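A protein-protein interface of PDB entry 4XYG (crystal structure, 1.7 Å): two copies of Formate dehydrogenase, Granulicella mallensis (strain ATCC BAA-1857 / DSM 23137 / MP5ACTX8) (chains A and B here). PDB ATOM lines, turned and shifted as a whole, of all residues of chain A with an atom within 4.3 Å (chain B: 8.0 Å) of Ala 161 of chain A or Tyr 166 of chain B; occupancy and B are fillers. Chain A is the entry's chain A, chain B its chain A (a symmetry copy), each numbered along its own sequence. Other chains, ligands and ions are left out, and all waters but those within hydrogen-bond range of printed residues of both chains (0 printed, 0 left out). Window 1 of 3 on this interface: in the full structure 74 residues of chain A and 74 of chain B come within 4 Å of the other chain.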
ATOM      1  N   MET A 157      -6.710  18.640  13.169  1.00  0.00           N
ATOM      2  CA  MET A 157      -7.534  17.720  13.960  1.00  0.00           C
ATOM      3  C   MET A 157      -7.957  16.551  13.068  1.00  0.00           C
ATOM      4  O   MET A 157      -7.860  15.381  13.470  1.00  0.00           O
ATOM      5  CB  MET A 157      -8.765  18.457  14.495  1.00  0.00           C
ATOM      6  CG  MET A 157      -9.799  17.598  15.217  1.00  0.00           C
ATOM      7  SD  MET A 157     -11.301  18.580  15.499  1.00  0.00           S
ATOM      8  CE  MET A 157     -11.983  18.603  13.853  1.00  0.00           C
ATOM      9  N   MET A 158      -8.413  16.857  11.856  1.00  0.00           N
ATOM     10  CA  MET A 158      -8.829  15.802  10.928  1.00  0.00           C
ATOM     11  C   MET A 158      -7.695  14.878  10.498  1.00  0.00           C
ATOM     12  O   MET A 158      -7.898  13.671  10.398  1.00  0.00           O
ATOM     13  CB  MET A 158      -9.543  16.391   9.710  1.00  0.00           C
ATOM     14  CG  MET A 158     -10.919  16.879  10.106  1.00  0.00           C
ATOM     15  SD  MET A 158     -11.685  17.719   8.713  1.00  0.00           S
ATOM     16  CE  MET A 158     -13.388  17.736   9.271  1.00  0.00           C
ATOM     17  N   ILE A 159      -6.519  15.444  10.234  1.00  0.00           N
ATOM     18  CA  ILE A 159      -5.342  14.636   9.908  1.00  0.00           C
ATOM     19  C   ILE A 159      -5.050  13.621  11.016  1.00  0.00           C
ATOM     20  O   ILE A 159      -4.903  12.423  10.744  1.00  0.00           O
ATOM     21  CB  ILE A 159      -4.095  15.511   9.687  1.00  0.00           C
ATOM     22  CG1 ILE A 159      -4.271  16.348   8.419  1.00  0.00           C
ATOM     23  CG2 ILE A 159      -2.835  14.637   9.591  1.00  0.00           C
ATOM     24  CD1 ILE A 159      -3.198  17.410   8.229  1.00  0.00           C
ATOM     25  N   LEU A 160      -4.951  14.088  12.254  1.00  0.00           N
ATOM     26  CA  LEU A 160      -4.679  13.179  13.371  1.00  0.00           C
ATOM     27  C   LEU A 160      -5.773  12.110  13.515  1.00  0.00           C
ATOM     28  O   LEU A 160      -5.483  10.938  13.723  1.00  0.00           O
ATOM     29  CB  LEU A 160      -4.534  13.953  14.683  1.00  0.00           C
ATOM     30  CG  LEU A 160      -3.254  14.784  14.779  1.00  0.00           C
ATOM     31  CD1 LEU A 160      -3.410  15.812  15.891  1.00  0.00           C
ATOM     32  CD2 LEU A 160      -2.063  13.868  15.054  1.00  0.00           C
ATOM     33  N   ALA A 161      -7.032  12.510  13.392  1.00  0.00           N
ATOM     34  CA  ALA A 161      -8.130  11.553  13.571  1.00  0.00           C
ATOM     35  C   ALA A 161      -8.083  10.444  12.530  1.00  0.00           C
ATOM     36  O   ALA A 161      -8.342   9.275  12.857  1.00  0.00           O
ATOM     37  CB  ALA A 161      -9.480  12.265  13.517  1.00  0.00           C
ATOM     38  N   LEU A 162      -7.767  10.799  11.287  1.00  0.00           N
ATOM     39  CA  LEU A 162      -7.708   9.809  10.205  1.00  0.00           C
ATOM     40  C   LEU A 162      -6.550   8.831  10.419  1.00  0.00           C
ATOM     41  O   LEU A 162      -6.734   7.608  10.411  1.00  0.00           O
ATOM     42  CB  LEU A 162      -7.544  10.486   8.848  1.00  0.00           C
ATOM     43  CG  LEU A 162      -8.742  11.223   8.259  1.00  0.00           C
ATOM     44  CD1 LEU A 162      -8.334  11.787   6.910  1.00  0.00           C
ATOM     45  CD2 LEU A 162      -9.918  10.273   8.128  1.00  0.00           C
ATOM     46  N   VAL A 163      -5.356   9.374  10.615  1.00  0.00           N
ATOM     47  CA  VAL A 163      -4.156   8.541  10.690  1.00  0.00           C
ATOM     48  C   VAL A 163      -4.216   7.581  11.890  1.00  0.00           C
ATOM     49  O   VAL A 163      -3.821   6.412  11.768  1.00  0.00           O
ATOM     50  CB  VAL A 163      -2.877   9.410  10.685  1.00  0.00           C
ATOM     51  CG1 VAL A 163      -1.633   8.563  10.929  1.00  0.00           C
ATOM     52  CG2 VAL A 163      -2.751  10.154   9.348  1.00  0.00           C
ATOM     53  N   ARG A 164      -4.751   8.049  13.017  1.00  0.00           N
ATOM     54  CA  ARG A 164      -4.785   7.256  14.261  1.00  0.00           C
ATOM     55  C   ARG A 164      -6.018   6.358  14.398  1.00  0.00           C
ATOM     56  O   ARG A 164      -6.115   5.570  15.338  1.00  0.00           O
ATOM     57  CB  ARG A 164      -4.641   8.152  15.501  1.00  0.00           C
ATOM     58  CG  ARG A 164      -3.377   9.013  15.515  1.00  0.00           C
ATOM     59  CD  ARG A 164      -3.056   9.514  16.929  1.00  0.00           C
ATOM     60  NE  ARG A 164      -2.841   8.369  17.816  1.00  0.00           N
ATOM     61  CZ  ARG A 164      -1.705   7.681  17.905  1.00  0.00           C
ATOM     62  NH1 ARG A 164      -0.634   8.040  17.209  1.00  0.00           N
ATOM     63  NH2 ARG A 164      -1.646   6.624  18.693  1.00  0.00           N
ATOM     64  N   ASN A 165      -6.953   6.473  13.454  1.00  0.00           N
ATOM     65  CA  ASN A 165      -8.195   5.673  13.485  1.00  0.00           C
ATOM     66  C   ASN A 165      -9.137   6.007  14.655  1.00  0.00           C
ATOM     67  O   ASN A 165      -9.775   5.119  15.243  1.00  0.00           O
ATOM     68  CB  ASN A 165      -7.896   4.160  13.428  1.00  0.00           C
ATOM     69  CG  ASN A 165      -9.070   3.352  12.892  1.00  0.00           C
ATOM     70  OD1 ASN A 165      -9.736   3.774  11.949  1.00  0.00           O
ATOM     71  ND2 ASN A 165      -9.326   2.192  13.489  1.00  0.00           N
ATOM     72  N   TYR A 166      -9.248   7.301  14.967  1.00  0.00           N
ATOM     73  CA  TYR A 166     -10.022   7.776  16.109  1.00  0.00           C
ATOM     74  C   TYR A 166     -11.502   7.459  15.994  1.00  0.00           C
ATOM     75  O   TYR A 166     -12.094   6.941  16.935  1.00  0.00           O
ATOM     76  CB  TYR A 166      -9.843   9.300  16.253  1.00  0.00           C
ATOM     77  CG  TYR A 166     -10.355   9.957  17.533  1.00  0.00           C
ATOM     78  CD1 TYR A 166     -10.724   9.213  18.649  1.00  0.00           C
ATOM     79  CD2 TYR A 166     -10.463  11.344  17.618  1.00  0.00           C
ATOM     80  CE1 TYR A 166     -11.177   9.830  19.817  1.00  0.00           C
ATOM     81  CE2 TYR A 166     -10.916  11.966  18.773  1.00  0.00           C
ATOM     82  CZ  TYR A 166     -11.274  11.207  19.868  1.00  0.00           C
ATOM     83  OH  TYR A 166     -11.714  11.824  21.015  1.00  0.00           O
ATOM     84  N   LEU A 167     -12.115   7.823  14.869  1.00  0.00           N
ATOM     85  CA  LEU A 167     -13.576   7.794  14.785  1.00  0.00           C
ATOM     86  C   LEU A 167     -14.188   6.397  14.980  1.00  0.00           C
ATOM     87  O   LEU A 167     -15.137   6.252  15.751  1.00  0.00           O
ATOM     88  CB  LEU A 167     -14.083   8.476  13.501  1.00  0.00           C
ATOM     89  CG  LEU A 167     -13.566   9.912  13.359  1.00  0.00           C
ATOM     90  CD1 LEU A 167     -14.014  10.520  12.057  1.00  0.00           C
ATOM     91  CD2 LEU A 167     -14.040  10.777  14.504  1.00  0.00           C
ATOM     92  N   GLY A 329     -13.855  11.139   7.565  1.00  0.00           N
ATOM     93  CA  GLY A 329     -13.934  11.914   8.788  1.00  0.00           C
ATOM     94  C   GLY A 329     -14.674  13.228   8.612  1.00  0.00           C
ATOM     95  O   GLY A 329     -14.334  14.231   9.258  1.00  0.00           O
ATOM     96  N   THR A 331     -17.271  16.466   8.484  1.00  0.00           N
ATOM     97  CA  THR A 331     -18.259  17.205   9.262  1.00  0.00           C
ATOM     98  C   THR A 331     -19.022  18.090   8.278  1.00  0.00           C
ATOM     99  O   THR A 331     -18.566  18.296   7.152  1.00  0.00           O
ATOM    100  CB  THR A 331     -17.639  18.125  10.339  1.00  0.00           C
ATOM    101  OG1 THR A 331     -16.886  19.163   9.703  1.00  0.00           O
ATOM    102  CG2 THR A 331     -16.742  17.351  11.315  1.00  0.00           C
ATOM    103  N   GLU B 153       0.515  12.132  20.601  1.00  0.00           N
ATOM    104  CA  GLU B 153      -0.362  12.422  19.469  1.00  0.00           C
ATOM    105  C   GLU B 153      -1.823  12.175  19.795  1.00  0.00           C
ATOM    106  O   GLU B 153      -2.682  12.977  19.442  1.00  0.00           O
ATOM    107  CB  GLU B 153       0.015  11.582  18.248  1.00  0.00           C
ATOM    108  CG  GLU B 153       1.364  11.918  17.622  1.00  0.00           C
ATOM    109  CD  GLU B 153       1.597  11.115  16.358  1.00  0.00           C
ATOM    110  OE1 GLU B 153       0.646  10.431  15.916  1.00  0.00           O
ATOM    111  OE2 GLU B 153       2.706  11.184  15.791  1.00  0.00           O
ATOM    112  N   HIS B 154      -2.114  11.045  20.434  1.00  0.00           N
ATOM    113  CA  HIS B 154      -3.483  10.715  20.810  1.00  0.00           C
ATOM    114  C   HIS B 154      -4.064  11.794  21.724  1.00  0.00           C
ATOM    115  O   HIS B 154      -5.217  12.189  21.558  1.00  0.00           O
ATOM    116  CB  HIS B 154      -3.490   9.370  21.535  1.00  0.00           C
ATOM    117  CG  HIS B 154      -4.677   8.507  21.246  1.00  0.00           C
ATOM    118  ND1 HIS B 154      -4.809   7.793  20.073  1.00  0.00           N
ATOM    119  CD2 HIS B 154      -5.754   8.193  22.005  1.00  0.00           C
ATOM    120  CE1 HIS B 154      -5.931   7.088  20.118  1.00  0.00           C
ATOM    121  NE2 HIS B 154      -6.519   7.317  21.276  1.00  0.00           N
ATOM    122  N   MET B 157      -4.763  15.034  19.756  1.00  0.00           N
ATOM    123  CA  MET B 157      -5.904  14.744  18.884  1.00  0.00           C
ATOM    124  C   MET B 157      -7.190  14.859  19.705  1.00  0.00           C
ATOM    125  O   MET B 157      -8.167  15.489  19.267  1.00  0.00           O
ATOM    126  CB  MET B 157      -5.766  13.333  18.303  1.00  0.00           C
ATOM    127  CG  MET B 157      -6.953  12.824  17.489  1.00  0.00           C
ATOM    128  SD  MET B 157      -6.732  11.052  17.155  1.00  0.00           S
ATOM    129  CE  MET B 157      -7.116  10.373  18.756  1.00  0.00           C
ATOM    130  N   MET B 158      -7.194  14.271  20.898  1.00  0.00           N
ATOM    131  CA  MET B 158      -8.377  14.341  21.760  1.00  0.00           C
ATOM    132  C   MET B 158      -8.719  15.752  22.222  1.00  0.00           C
ATOM    133  O   MET B 158      -9.894  16.111  22.265  1.00  0.00           O
ATOM    134  CB  MET B 158      -8.245  13.393  22.954  1.00  0.00           C
ATOM    135  CG  MET B 158      -8.403  11.961  22.494  1.00  0.00           C
ATOM    136  SD  MET B 158      -8.079  10.847  23.869  1.00  0.00           S
ATOM    137  CE  MET B 158      -8.794   9.341  23.211  1.00  0.00           C
ATOM    138  N   ILE B 159      -7.703  16.537  22.577  1.00  0.00           N
ATOM    139  CA  ILE B 159      -7.917  17.938  22.943  1.00  0.00           C
ATOM    140  C   ILE B 159      -8.625  18.697  21.818  1.00  0.00           C
ATOM    141  O   ILE B 159      -9.644  19.358  22.054  1.00  0.00           O
ATOM    142  CB  ILE B 159      -6.591  18.648  23.271  1.00  0.00           C
ATOM    143  CG1 ILE B 159      -5.999  18.067  24.556  1.00  0.00           C
ATOM    144  CG2 ILE B 159      -6.812  20.162  23.410  1.00  0.00           C
ATOM    145  CD1 ILE B 159      -4.582  18.540  24.849  1.00  0.00           C
ATOM    146  N   LEU B 160      -8.089  18.621  20.607  1.00  0.00           N
ATOM    147  CA  LEU B 160      -8.711  19.315  19.475  1.00  0.00           C
ATOM    148  C   LEU B 160     -10.147  18.825  19.226  1.00  0.00           C
ATOM    149  O   LEU B 160     -11.049  19.619  18.993  1.00  0.00           O
ATOM    150  CB  LEU B 160      -7.878  19.144  18.204  1.00  0.00           C
ATOM    151  CG  LEU B 160      -6.558  19.914  18.215  1.00  0.00           C
ATOM    152  CD1 LEU B 160      -5.643  19.353  17.134  1.00  0.00           C
ATOM    153  CD2 LEU B 160      -6.824  21.399  17.978  1.00  0.00           C
ATOM    154  N   ALA B 161     -10.360  17.518  19.288  1.00  0.00           N
ATOM    155  CA  ALA B 161     -11.696  16.975  19.008  1.00  0.00           C
ATOM    156  C   ALA B 161     -12.726  17.479  20.008  1.00  0.00           C
ATOM    157  O   ALA B 161     -13.866  17.786  19.623  1.00  0.00           O
ATOM    158  CB  ALA B 161     -11.669  15.450  19.007  1.00  0.00           C
ATOM    159  N   LEU B 162     -12.343  17.554  21.280  1.00  0.00           N
ATOM    160  CA  LEU B 162     -13.264  18.013  22.326  1.00  0.00           C
ATOM    161  C   LEU B 162     -13.606  19.494  22.146  1.00  0.00           C
ATOM    162  O   LEU B 162     -14.779  19.881  22.098  1.00  0.00           O
ATOM    163  CB  LEU B 162     -12.669  17.804  23.715  1.00  0.00           C
ATOM    164  CG  LEU B 162     -12.583  16.382  24.259  1.00  0.00           C
ATOM    165  CD1 LEU B 162     -11.979  16.442  25.649  1.00  0.00           C
ATOM    166  CD2 LEU B 162     -13.965  15.756  24.283  1.00  0.00           C
ATOM    167  N   VAL B 163     -12.575  20.323  22.043  1.00  0.00           N
ATOM    168  CA  VAL B 163     -12.776  21.771  22.010  1.00  0.00           C
ATOM    169  C   VAL B 163     -13.586  22.194  20.773  1.00  0.00           C
ATOM    170  O   VAL B 163     -14.460  23.068  20.875  1.00  0.00           O
ATOM    171  CB  VAL B 163     -11.428  22.520  22.123  1.00  0.00           C
ATOM    172  CG1 VAL B 163     -11.611  24.021  21.923  1.00  0.00           C
ATOM    173  CG2 VAL B 163     -10.788  22.247  23.492  1.00  0.00           C
ATOM    174  N   ARG B 164     -13.341  21.547  19.633  1.00  0.00           N
ATOM    175  CA  ARG B 164     -13.989  21.921  18.362  1.00  0.00           C
ATOM    176  C   ARG B 164     -15.334  21.230  18.118  1.00  0.00           C
ATOM    177  O   ARG B 164     -16.024  21.533  17.145  1.00  0.00           O
ATOM    178  CB  ARG B 164     -13.052  21.692  17.167  1.00  0.00           C
ATOM    179  CG  ARG B 164     -11.716  22.432  17.260  1.00  0.00           C
ATOM    180  CD  ARG B 164     -11.040  22.544  15.887  1.00  0.00           C
ATOM    181  NE  ARG B 164     -11.912  23.285  14.974  1.00  0.00           N
ATOM    182  CZ  ARG B 164     -12.012  24.612  14.927  1.00  0.00           C
ATOM    183  NH1 ARG B 164     -11.254  25.380  15.700  1.00  0.00           N
ATOM    184  NH2 ARG B 164     -12.880  25.169  14.106  1.00  0.00           N
ATOM    185  N   ASN B 165     -15.707  20.310  19.007  1.00  0.00           N
ATOM    186  CA  ASN B 165     -16.976  19.563  18.873  1.00  0.00           C
ATOM    187  C   ASN B 165     -17.029  18.616  17.661  1.00  0.00           C
ATOM    188  O   ASN B 165     -18.072  18.468  17.004  1.00  0.00           O
ATOM    189  CB  ASN B 165     -18.195  20.509  18.892  1.00  0.00           C
ATOM    190  CG  ASN B 165     -19.474  19.806  19.326  1.00  0.00           C
ATOM    191  OD1 ASN B 165     -19.452  18.986  20.242  1.00  0.00           O
ATOM    192  ND2 ASN B 165     -20.587  20.122  18.672  1.00  0.00           N
ATOM    193  N   TYR B 166     -15.906  17.945  17.391  1.00  0.00           N
ATOM    194  CA  TYR B 166     -15.761  17.083  16.223  1.00  0.00           C
ATOM    195  C   TYR B 166     -16.713  15.901  16.237  1.00  0.00           C
ATOM    196  O   TYR B 166     -17.384  15.642  15.244  1.00  0.00           O
ATOM    197  CB  TYR B 166     -14.312  16.561  16.146  1.00  0.00           C
ATOM    198  CG  TYR B 166     -13.878  15.857  14.863  1.00  0.00           C
ATOM    199  CD1 TYR B 166     -14.641  15.904  13.700  1.00  0.00           C
ATOM    200  CD2 TYR B 166     -12.685  15.138  14.823  1.00  0.00           C
ATOM    201  CE1 TYR B 166     -14.223  15.265  12.531  1.00  0.00           C
ATOM    202  CE2 TYR B 166     -12.263  14.497  13.667  1.00  0.00           C
ATOM    203  CZ  TYR B 166     -13.035  14.560  12.525  1.00  0.00           C
ATOM    204  OH  TYR B 166     -12.613  13.932  11.378  1.00  0.00           O
ATOM    205  N   LEU B 167     -16.730  15.149  17.336  1.00  0.00           N
ATOM    206  CA  LEU B 167     -17.416  13.855  17.332  1.00  0.00           C
ATOM    207  C   LEU B 167     -18.925  13.946  17.048  1.00  0.00           C
ATOM    208  O   LEU B 167     -19.433  13.194  16.217  1.00  0.00           O
ATOM    209  CB  LEU B 167     -17.111  13.049  18.607  1.00  0.00           C
ATOM    210  CG  LEU B 167     -15.608  12.857  18.832  1.00  0.00           C
ATOM    211  CD1 LEU B 167     -15.344  12.137  20.127  1.00  0.00           C
ATOM    212  CD2 LEU B 167     -14.980  12.087  17.694  1.00  0.00           C
ATOM    213  N   PRO B 168     -19.636  14.872  17.716  1.00  0.00           N
ATOM    214  CA  PRO B 168     -21.065  14.998  17.390  1.00  0.00           C
ATOM    215  C   PRO B 168     -21.308  15.537  15.985  1.00  0.00           C
ATOM    216  O   PRO B 168     -22.310  15.189  15.355  1.00  0.00           O
ATOM    217  CB  PRO B 168     -21.560  16.020  18.418  1.00  0.00           C
ATOM    218  CG  PRO B 168     -20.584  15.927  19.550  1.00  0.00           C
ATOM    219  CD  PRO B 168     -19.271  15.724  18.862  1.00  0.00           C
ATOM    220  N   SER B 169     -20.407  16.382  15.498  1.00  0.00           N
ATOM    221  CA  SER B 169     -20.533  16.932  14.155  1.00  0.00           C
ATOM    222  C   SER B 169     -20.326  15.878  13.068  1.00  0.00           C
ATOM    223  O   SER B 169     -20.973  15.928  12.028  1.00  0.00           O
ATOM    224  CB  SER B 169     -19.561  18.099  13.962  1.00  0.00           C
ATOM    225  OG  SER B 169     -19.797  19.089  14.946  1.00  0.00           O
ATOM    226  N   HIS B 170     -19.417  14.932  13.299  1.00  0.00           N
ATOM    227  CA  HIS B 170     -19.220  13.833  12.357  1.00  0.00           C
ATOM    228  C   HIS B 170     -20.470  12.969  12.301  1.00  0.00           C
ATOM    229  O   HIS B 170     -20.886  12.526  11.229  1.00  0.00           O
ATOM    230  CB  HIS B 170     -18.034  12.951  12.762  1.00  0.00           C
ATOM    231  CG  HIS B 170     -17.839  11.766  11.868  1.00  0.00           C
ATOM    232  ND1 HIS B 170     -17.533  11.884  10.528  1.00  0.00           N
ATOM    233  CD2 HIS B 170     -17.913  10.435  12.118  1.00  0.00           C
ATOM    234  CE1 HIS B 170     -17.427  10.680   9.993  1.00  0.00           C
ATOM    235  NE2 HIS B 170     -17.653   9.784  10.938  1.00  0.00           N
ATOM    236  N   LYS B 171     -21.059  12.719  13.463  1.00  0.00           N
ATOM    237  CA  LYS B 171     -22.282  11.921  13.521  1.00  0.00           C
ATOM    238  C   LYS B 171     -23.397  12.555  12.675  1.00  0.00           C
ATOM    239  O   LYS B 171     -24.090  11.862  11.929  1.00  0.00           O
ATOM    240  CB  LYS B 171     -22.736  11.718  14.972  1.00  0.00           C
ATOM    241  CG  LYS B 171     -23.944  10.787  15.107  1.00  0.00           C
ATOM    242  CD  LYS B 171     -24.541  10.866  16.505  1.00  0.00           C
ATOM    243  CE  LYS B 171     -25.857  10.104  16.605  1.00  0.00           C
ATOM    244  NZ  LYS B 171     -25.677   8.755  17.202  1.00  0.00           N
ATOM    245  N   ILE B 172     -23.543  13.873  12.764  1.00  0.00           N
ATOM    246  CA  ILE B 172     -24.531  14.588  11.949  1.00  0.00           C
ATOM    247  C   ILE B 172     -24.260  14.417  10.445  1.00  0.00           C
ATOM    248  O   ILE B 172     -25.187  14.200   9.660  1.00  0.00           O
ATOM    249  CB  ILE B 172     -24.619  16.083  12.366  1.00  0.00           C
ATOM    250  CG1 ILE B 172     -25.276  16.209  13.740  1.00  0.00           C
ATOM    251  CG2 ILE B 172     -25.397  16.923  11.335  1.00  0.00           C
ATOM    252  CD1 ILE B 172     -25.186  17.603  14.342  1.00  0.00           C
ATOM    253  N   ALA B 173     -22.994  14.477  10.038  1.00  0.00           N
ATOM    254  CA  ALA B 173     -22.654  14.249   8.635  1.00  0.00           C
ATOM    255  C   ALA B 173     -23.037  12.846   8.179  1.00  0.00           C
ATOM    256  O   ALA B 173     -23.645  12.680   7.119  1.00  0.00           O
ATOM    257  CB  ALA B 173     -21.164  14.512   8.373  1.00  0.00           C
ATOM    258  N   CYS B 183     -23.964  22.035  15.192  1.00  0.00           N
ATOM    259  CA  CYS B 183     -22.555  21.644  15.199  1.00  0.00           C
ATOM    260  C   CYS B 183     -21.696  22.662  15.937  1.00  0.00           C
ATOM    261  O   CYS B 183     -20.825  22.300  16.724  1.00  0.00           O
ATOM    262  CB  CYS B 183     -22.023  21.490  13.769  1.00  0.00           C
ATOM    263  SG  CYS B 183     -22.737  20.155  12.776  1.00  0.00           S
ATOM    264  N   ARG B 186     -21.302  24.224  20.345  1.00  0.00           N
ATOM    265  CA  ARG B 186     -20.289  23.891  21.344  1.00  0.00           C
ATOM    266  C   ARG B 186     -18.888  23.846  20.747  1.00  0.00           C
ATOM    267  O   ARG B 186     -18.003  23.199  21.309  1.00  0.00           O
ATOM    268  CB  ARG B 186     -20.581  22.524  21.990  1.00  0.00           C
ATOM    269  CG  ARG B 186     -21.968  22.358  22.578  1.00  0.00           C
ATOM    270  CD  ARG B 186     -22.139  20.935  23.115  1.00  0.00           C
ATOM    271  NE  ARG B 186     -21.070  20.596  24.051  1.00  0.00           N
ATOM    272  CZ  ARG B 186     -21.077  20.944  25.334  1.00  0.00           C
ATOM    273  NH1 ARG B 186     -22.097  21.639  25.816  1.00  0.00           N
ATOM    274  NH2 ARG B 186     -20.067  20.606  26.137  1.00  0.00           N
ATOM    275  N   SER B 187     -18.680  24.538  19.627  1.00  0.00           N
ATOM    276  CA  SER B 187     -17.401  24.475  18.898  1.00  0.00           C
ATOM    277  C   SER B 187     -16.559  25.719  19.151  1.00  0.00           C
ATOM    278  O   SER B 187     -16.981  26.838  18.831  1.00  0.00           O
ATOM    279  CB  SER B 187     -17.652  24.298  17.402  1.00  0.00           C
ATOM    280  OG  SER B 187     -16.435  24.212  16.671  1.00  0.00           O
ATOM    281  N   TYR B 188     -15.372  25.519  19.721  1.00  0.00           N
ATOM    282  CA  TYR B 188     -14.455  26.620  20.029  1.00  0.00           C
ATOM    283  C   TYR B 188     -13.114  26.351  19.367  1.00  0.00           C
ATOM    284  O   TYR B 188     -12.804  25.211  19.034  1.00  0.00           O
ATOM    285  CB  TYR B 188     -14.239  26.745  21.547  1.00  0.00           C
ATOM    286  CG  TYR B 188     -15.500  27.055  22.314  1.00  0.00           C
ATOM    287  CD1 TYR B 188     -15.935  28.361  22.463  1.00  0.00           C
ATOM    288  CD2 TYR B 188     -16.252  26.038  22.883  1.00  0.00           C
ATOM    289  CE1 TYR B 188     -17.085  28.651  23.158  1.00  0.00           C
ATOM    290  CE2 TYR B 188     -17.424  26.314  23.575  1.00  0.00           C
ATOM    291  CZ  TYR B 188     -17.827  27.627  23.709  1.00  0.00           C
ATOM    292  OH  TYR B 188     -18.988  27.929  24.399  1.00  0.00           O
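Printed residues of chain B that touch a printed residue of chain A: Glu 153, His 154, Met 157, Met 158, Leu 160, Ala 161, Arg 164, Tyr 166, Leu 167, Ser 169 and His 170.
Hydrophobic or aromatic side chains of chain B that line the printed part of chain A: His 154, Met 157, Met 158, Leu 160, Ala 161, Tyr 166, Leu 167 and His 170.
Hydrophobic or aromatic side chains of chain A that line the printed part of chain B: Met 157, Met 158, Leu 160, Ala 161, Tyr 166 and Leu 167.
Among the printed residues, pairs that only touch across the chains: Met 157 of chain A with Tyr 166 of chain B (3.5 Å), Tyr 166 of chain A with Met 157 of chain B (3.5 Å), Thr 331 of chain A with Tyr 166 of chain B (3.5 Å), Ala 161 of chain A with Tyr 166 of chain B (3.6 Å), Tyr 166 of chain A with Ala 161 of chain B (3.6 Å), Leu 167 of chain A with Leu 167 of chain B (3.6 Å), Tyr 166 of chain A with Met 158 of chain B (3.6 Å), Met 158 of chain A with Tyr 166 of chain B (3.6 Å), Gly 329 of chain A with His 170 of chain B (3.7 Å), Tyr 166 of chain A with Leu 167 of chain B (3.8 Å), Leu 167 of chain A with Tyr 166 of chain B (3.8 Å), Leu 167 of chain A with His 170 of chain B (3.9 Å), Met 157 of chain A with Ala 161 of chain B (3.9 Å), Ala 161 of chain A with Met 157 of chain B (3.9 Å), Thr 331 of chain A with Ser 169 of chain B (3.9 Å), Arg 164 of chain A with Met 157 of chain B (3.9 Å) and Met 157 of chain A with Arg 164 of chain B (3.9 Å).
The backbone carbonyl oxygen of Leu 160 of chain A sits close to the side-chain sulfur of Met 157 of chain B.
The guanidinium group (NH1) of Arg 164 of chain A lies within salt-bridge range of the side-chain carboxylate (OE1) of Glu 153 of chain B, 3.0 Å away.
O of Gly 329 of chain A lies within hydrogen-bond range of OH of Tyr 166 of chain B (2.7 Å).
The guanidinium group of Arg 164 of chain A lies within hydrogen-bond range of a ring nitrogen (ND1) of His 154 of chain B (3.0 Å).
O of Leu 160 of chain B lies close to SD of Met 157 of chain A, 3.7 Å away.
Met 157 of chain A touches Ala 161 of chain B, and with the chains exchanged Ala 161 of chain A touches Met 157 of chain B.
Met 157 of chain A touches Tyr 166 of chain B, and with the chains exchanged Tyr 166 of chain A touches Met 157 of chain B.
Met 158 of chain A touches Tyr 166 of chain B, and with the chains exchanged Tyr 166 of chain A touches Met 158 of chain B.
Tyr 166 of chain A touches Leu 167 of chain B, and with the chains exchanged Leu 167 of chain A touches Tyr 166 of chain B.
Positions printed for both chains: 157, 158, 159, 160, 161, 162, 163, 164, 165, 166 and 167.
Of chain B, only Met 157 and Tyr 166 come within 4 Å of Ala 161 of chain A.
Of the printed residues of chain A, Leu 160 of chain B touches Met 157.
Leu 162 of chain B touches none of the printed residues of chain A.
Tyr 166 of chain B touches just these residues of chain A: Met 157, Met 158, Ala 161, Leu 167, Gly 329 and Thr 331.
Printed residues of chain A within 4 Å of Ser 169 of chain B: Thr 331 (3.9 Å).
Tyr 188 of chain B touches none of the printed residues of chain A.
The nearest printed residue of chain A that does not touch Tyr 166 of chain B is Tyr 166 of chain A (5.2 Å).
O of Asn 165 of chain B lies within hydrogen-bond range of OG of Ser 169 of chain B, at 2.8 Å.
O of Arg 164 of chain B lies within hydrogen-bond range of OG of Ser 187 of chain B.
The backbone carbonyl oxygen of Ala 161 of chain B lies within hydrogen-bond range of the backbone NH of Tyr 166 of chain B (3.0 Å).
The backbone carbonyl oxygen (O) of Ala 161 of chain A sits at hydrogen-bond distance from the backbone NH (N) of Tyr 166 of chain A, 3.0 Å away.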
